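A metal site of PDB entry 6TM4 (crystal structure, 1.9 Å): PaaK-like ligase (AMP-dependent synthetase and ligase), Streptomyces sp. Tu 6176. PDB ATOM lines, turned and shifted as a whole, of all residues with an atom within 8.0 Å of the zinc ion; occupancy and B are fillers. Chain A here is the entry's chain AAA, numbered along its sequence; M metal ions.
The zinc ion is bound by a ring nitrogen (NE2) of His 254 (2.0 Å), the side-chain sulfur of Cys 310 (2.3 Å), the side-chain sulfur of Cys 248 (2.4 Å) and the side-chain sulfur of Cys 308 (2.5 Å).
ND1 of His 254 lies within hydrogen-bond range of O of Leu 314, at 2.6 Å.
The backbone NH (N) of His 254 lies within hydrogen-bond range of the backbone carbonyl oxygen (O) of Gly 246, at 2.8 Å.
The backbone NH (N) of Trp 312 lies close to the side-chain sulfur (SG) of Cys 310 (3.5 Å).
The side-chain sulfur (SG) of Cys 248 lies close to the backbone carbonyl oxygen (O) of Arg 252 (3.6 Å).
The side-chain sulfur of Cys 248 sits close to the backbone NH of Glu 250.
The side-chain sulfur (SG) of Cys 248 lies close to the backbone NH (N) of Gly 251 (3.7 Å).
SG of Cys 308 sits close to NE of Arg 252 (3.7 Å).
Within 4 Å of the zinc ion: Cys 248, His 254, Cys 308 and Cys 310.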
ATOM      1  N   GLY A 246      21.188  12.940  25.061  1.00  0.00           N
ATOM      2  CA  GLY A 246      22.276  13.318  24.131  1.00  0.00           C
ATOM      3  C   GLY A 246      22.892  12.070  23.510  1.00  0.00           C
ATOM      4  O   GLY A 246      22.913  11.014  24.190  1.00  0.00           O
ATOM      5  N   GLN A 247      23.409  12.216  22.304  1.00  0.00           N
ATOM      6  CA  GLN A 247      24.063  11.129  21.534  1.00  0.00           C
ATOM      7  C   GLN A 247      25.372  10.744  22.232  1.00  0.00           C
ATOM      8  O   GLN A 247      26.016  11.618  22.803  1.00  0.00           O
ATOM      9  CB  GLN A 247      24.315  11.653  20.107  1.00  0.00           C
ATOM     10  CG  GLN A 247      24.794  10.633  19.094  1.00  0.00           C
ATOM     11  CD  GLN A 247      25.131  11.360  17.800  1.00  0.00           C
ATOM     12  OE1 GLN A 247      26.283  11.796  17.558  1.00  0.00           O
ATOM     13  NE2 GLN A 247      24.097  11.512  16.986  1.00  0.00           N
ATOM     14  N   CYS A 248      25.727   9.461  22.220  1.00  0.00           N
ATOM     15  CA  CYS A 248      27.077   8.956  22.594  1.00  0.00           C
ATOM     16  C   CYS A 248      27.908   8.776  21.311  1.00  0.00           C
ATOM     17  O   CYS A 248      27.383   8.871  20.197  1.00  0.00           O
ATOM     18  CB  CYS A 248      26.970   7.647  23.356  1.00  0.00           C
ATOM     19  SG  CYS A 248      26.466   6.291  22.234  1.00  0.00           S
ATOM     20  N   PRO A 249      29.244   8.503  21.410  1.00  0.00           N
ATOM     21  CA  PRO A 249      30.048   8.290  20.202  1.00  0.00           C
ATOM     22  C   PRO A 249      29.597   7.084  19.360  1.00  0.00           C
ATOM     23  O   PRO A 249      30.049   6.997  18.248  1.00  0.00           O
ATOM     24  CB  PRO A 249      31.466   8.073  20.761  1.00  0.00           C
ATOM     25  CG  PRO A 249      31.440   8.663  22.154  1.00  0.00           C
ATOM     26  CD  PRO A 249      30.028   8.414  22.650  1.00  0.00           C
ATOM     27  N   GLU A 250      28.734   6.203  19.880  1.00  0.00           N
ATOM     28  CA  GLU A 250      28.196   5.017  19.135  1.00  0.00           C
ATOM     29  C   GLU A 250      26.969   5.404  18.304  1.00  0.00           C
ATOM     30  O   GLU A 250      26.561   4.594  17.466  1.00  0.00           O
ATOM     31  CB  GLU A 250      27.818   3.878  20.083  1.00  0.00           C
ATOM     32  CG  GLU A 250      28.903   3.447  21.057  1.00  0.00           C
ATOM     33  CD  GLU A 250      29.956   2.494  20.519  1.00  0.00           C
ATOM     34  OE1 GLU A 250      31.106   2.931  20.335  1.00  0.00           O
ATOM     35  OE2 GLU A 250      29.639   1.300  20.311  1.00  0.00           O
ATOM     36  N   GLY A 251      26.390   6.588  18.526  1.00  0.00           N
ATOM     37  CA  GLY A 251      25.223   7.088  17.762  1.00  0.00           C
ATOM     38  C   GLY A 251      23.880   6.746  18.400  1.00  0.00           C
ATOM     39  O   GLY A 251      22.867   6.951  17.713  1.00  0.00           O
ATOM     40  N   ARG A 252      23.832   6.266  19.652  1.00  0.00           N
ATOM     41  CA  ARG A 252      22.571   6.205  20.469  1.00  0.00           C
ATOM     42  C   ARG A 252      22.390   7.481  21.305  1.00  0.00           C
ATOM     43  O   ARG A 252      23.390   8.084  21.751  1.00  0.00           O
ATOM     44  CB  ARG A 252      22.555   4.973  21.381  1.00  0.00           C
ATOM     45  CG  ARG A 252      22.902   3.688  20.650  1.00  0.00           C
ATOM     46  CD  ARG A 252      22.104   2.467  21.060  1.00  0.00           C
ATOM     47  NE  ARG A 252      22.975   1.300  21.123  1.00  0.00           N
ATOM     48  CZ  ARG A 252      22.587   0.039  20.926  1.00  0.00           C
ATOM     49  NH1 ARG A 252      23.477  -0.931  21.012  1.00  0.00           N
ATOM     50  NH2 ARG A 252      21.328  -0.247  20.635  1.00  0.00           N
ATOM     51  N   MET A 253      21.148   7.916  21.488  1.00  0.00           N
ATOM     52  CA  MET A 253      20.772   8.989  22.436  1.00  0.00           C
ATOM     53  C   MET A 253      20.542   8.332  23.797  1.00  0.00           C
ATOM     54  O   MET A 253      19.717   7.402  23.854  1.00  0.00           O
ATOM     55  CB  MET A 253      19.479   9.707  22.023  1.00  0.00           C
ATOM     56  CG  MET A 253      19.635  11.227  21.925  1.00  0.00           C
ATOM     57  SD  MET A 253      18.721  11.914  20.535  1.00  0.00           S
ATOM     58  CE  MET A 253      19.169  10.709  19.284  1.00  0.00           C
ATOM     59  N   HIS A 254      21.229   8.826  24.833  1.00  0.00           N
ATOM     60  CA  HIS A 254      21.107   8.341  26.224  1.00  0.00           C
ATOM     61  C   HIS A 254      20.318   9.377  27.032  1.00  0.00           C
ATOM     62  O   HIS A 254      20.584  10.576  26.894  1.00  0.00           O
ATOM     63  CB  HIS A 254      22.500   8.090  26.800  1.00  0.00           C
ATOM     64  CG  HIS A 254      23.169   6.849  26.309  1.00  0.00           C
ATOM     65  ND1 HIS A 254      23.078   5.679  26.977  1.00  0.00           N
ATOM     66  CD2 HIS A 254      23.966   6.609  25.242  1.00  0.00           C
ATOM     67  CE1 HIS A 254      23.809   4.756  26.367  1.00  0.00           C
ATOM     68  NE2 HIS A 254      24.358   5.293  25.289  1.00  0.00           N
ATOM     69  N   ASP A 306      19.389  -1.714  27.830  1.00  0.00           N
ATOM     70  CA  ASP A 306      20.503  -2.545  27.307  1.00  0.00           C
ATOM     71  C   ASP A 306      21.801  -1.751  27.413  1.00  0.00           C
ATOM     72  O   ASP A 306      21.825  -0.574  27.063  1.00  0.00           O
ATOM     73  CB  ASP A 306      20.266  -2.967  25.849  1.00  0.00           C
ATOM     74  CG  ASP A 306      19.171  -4.045  25.648  1.00  0.00           C
ATOM     75  OD1 ASP A 306      18.706  -4.637  26.649  1.00  0.00           O
ATOM     76  OD2 ASP A 306      18.786  -4.295  24.477  1.00  0.00           O
ATOM     77  N   PRO A 307      22.925  -2.353  27.875  1.00  0.00           N
ATOM     78  CA  PRO A 307      24.189  -1.637  27.914  1.00  0.00           C
ATOM     79  C   PRO A 307      24.599  -1.200  26.506  1.00  0.00           C
ATOM     80  O   PRO A 307      24.299  -1.921  25.525  1.00  0.00           O
ATOM     81  CB  PRO A 307      25.202  -2.625  28.527  1.00  0.00           C
ATOM     82  CG  PRO A 307      24.524  -3.985  28.417  1.00  0.00           C
ATOM     83  CD  PRO A 307      23.032  -3.735  28.383  1.00  0.00           C
ATOM     84  N   CYS A 308      25.236  -0.023  26.430  1.00  0.00           N
ATOM     85  CA  CYS A 308      25.837   0.502  25.181  1.00  0.00           C
ATOM     86  C   CYS A 308      27.387   0.391  25.298  1.00  0.00           C
ATOM     87  O   CYS A 308      27.990   0.614  26.490  1.00  0.00           O
ATOM     88  CB  CYS A 308      25.432   1.960  24.955  1.00  0.00           C
ATOM     89  SG  CYS A 308      25.723   2.483  23.217  1.00  0.00           S
ATOM     90  N   GLY A 309      27.996   0.134  24.090  1.00  0.00           N
ATOM     91  CA  GLY A 309      29.462   0.127  23.890  1.00  0.00           C
ATOM     92  C   GLY A 309      30.153   1.388  24.402  1.00  0.00           C
ATOM     93  O   GLY A 309      31.328   1.262  24.791  1.00  0.00           O
ATOM     94  N   CYS A 310      29.470   2.543  24.448  1.00  0.00           N
ATOM     95  CA  CYS A 310      30.037   3.853  24.890  1.00  0.00           C
ATOM     96  C   CYS A 310      30.481   3.807  26.366  1.00  0.00           C
ATOM     97  O   CYS A 310      31.386   4.599  26.721  1.00  0.00           O
ATOM     98  CB  CYS A 310      29.063   5.002  24.673  1.00  0.00           C
ATOM     99  SG  CYS A 310      27.582   4.967  25.783  1.00  0.00           S
ATOM    100  N   GLY A 311      29.845   2.983  27.196  1.00  0.00           N
ATOM    101  CA  GLY A 311      30.225   2.795  28.613  1.00  0.00           C
ATOM    102  C   GLY A 311      29.489   3.743  29.551  1.00  0.00           C
ATOM    103  O   GLY A 311      29.611   3.573  30.782  1.00  0.00           O
ATOM    104  N   TRP A 312      28.701   4.694  29.036  1.00  0.00           N
ATOM    105  CA  TRP A 312      27.774   5.477  29.886  1.00  0.00           C
ATOM    106  C   TRP A 312      26.722   4.524  30.455  1.00  0.00           C
ATOM    107  O   TRP A 312      26.121   3.760  29.662  1.00  0.00           O
ATOM    108  CB  TRP A 312      27.072   6.593  29.118  1.00  0.00           C
ATOM    109  CG  TRP A 312      27.953   7.524  28.360  1.00  0.00           C
ATOM    110  CD1 TRP A 312      29.321   7.609  28.369  1.00  0.00           C
ATOM    111  CD2 TRP A 312      27.506   8.575  27.503  1.00  0.00           C
ATOM    112  NE1 TRP A 312      29.741   8.627  27.550  1.00  0.00           N
ATOM    113  CE2 TRP A 312      28.653   9.234  27.004  1.00  0.00           C
ATOM    114  CE3 TRP A 312      26.238   8.989  27.073  1.00  0.00           C
ATOM    115  CZ2 TRP A 312      28.573  10.275  26.092  1.00  0.00           C
ATOM    116  CZ3 TRP A 312      26.160  10.033  26.195  1.00  0.00           C
ATOM    117  CH2 TRP A 312      27.303  10.672  25.710  1.00  0.00           C
ATOM    118  N   LEU A 313      26.498   4.554  31.776  1.00  0.00           N
ATOM    119  CA  LEU A 313      25.496   3.691  32.433  1.00  0.00           C
ATOM    120  C   LEU A 313      24.163   4.455  32.466  1.00  0.00           C
ATOM    121  O   LEU A 313      23.720   4.895  33.554  1.00  0.00           O
ATOM    122  CB  LEU A 313      26.030   3.246  33.802  1.00  0.00           C
ATOM    123  CG  LEU A 313      27.171   2.215  33.735  1.00  0.00           C
ATOM    124  CD1 LEU A 313      27.665   1.846  35.130  1.00  0.00           C
ATOM    125  CD2 LEU A 313      26.760   0.946  32.982  1.00  0.00           C
ATOM    126  N   LEU A 314      23.581   4.629  31.274  1.00  0.00           N
ATOM    127  CA  LEU A 314      22.277   5.328  31.067  1.00  0.00           C
ATOM    128  C   LEU A 314      21.461   4.618  29.955  1.00  0.00           C
ATOM    129  O   LEU A 314      21.999   4.228  28.867  1.00  0.00           O
ATOM    130  CB  LEU A 314      22.550   6.774  30.653  1.00  0.00           C
ATOM    131  CG  LEU A 314      23.090   7.695  31.745  1.00  0.00           C
ATOM    132  CD1 LEU A 314      23.516   9.019  31.156  1.00  0.00           C
ATOM    133  CD2 LEU A 314      22.048   7.910  32.837  1.00  0.00           C
ATOM    134  N   PRO A 315      20.106   4.566  30.145  1.00  0.00           N
ATOM    135  CA  PRO A 315      19.204   4.015  29.130  1.00  0.00           C
ATOM    136  C   PRO A 315      19.277   4.841  27.847  1.00  0.00           C
ATOM    137  O   PRO A 315      19.586   6.050  27.892  1.00  0.00           O
ATOM    138  CB  PRO A 315      17.791   4.107  29.719  1.00  0.00           C
ATOM    139  CG  PRO A 315      17.991   4.400  31.197  1.00  0.00           C
ATOM    140  CD  PRO A 315      19.358   5.061  31.314  1.00  0.00           C
ATOM    141  N   THR A 316      19.019   4.162  26.721  1.00  0.00           N
ATOM    142  CA  THR A 316      18.949   4.764  25.374  1.00  0.00           C
ATOM    143  C   THR A 316      17.483   5.005  25.025  1.00  0.00           C
ATOM    144  O   THR A 316      16.606   4.350  25.615  1.00  0.00           O
ATOM    145  CB  THR A 316      19.628   3.877  24.330  1.00  0.00           C
ATOM    146  OG1 THR A 316      18.881   2.662  24.323  1.00  0.00           O
ATOM    147  CG2 THR A 316      21.091   3.640  24.632  1.00  0.00           C
HETATM  148 ZN    ZN M   1      25.921   4.838  24.126  1.00  0.00          ZN
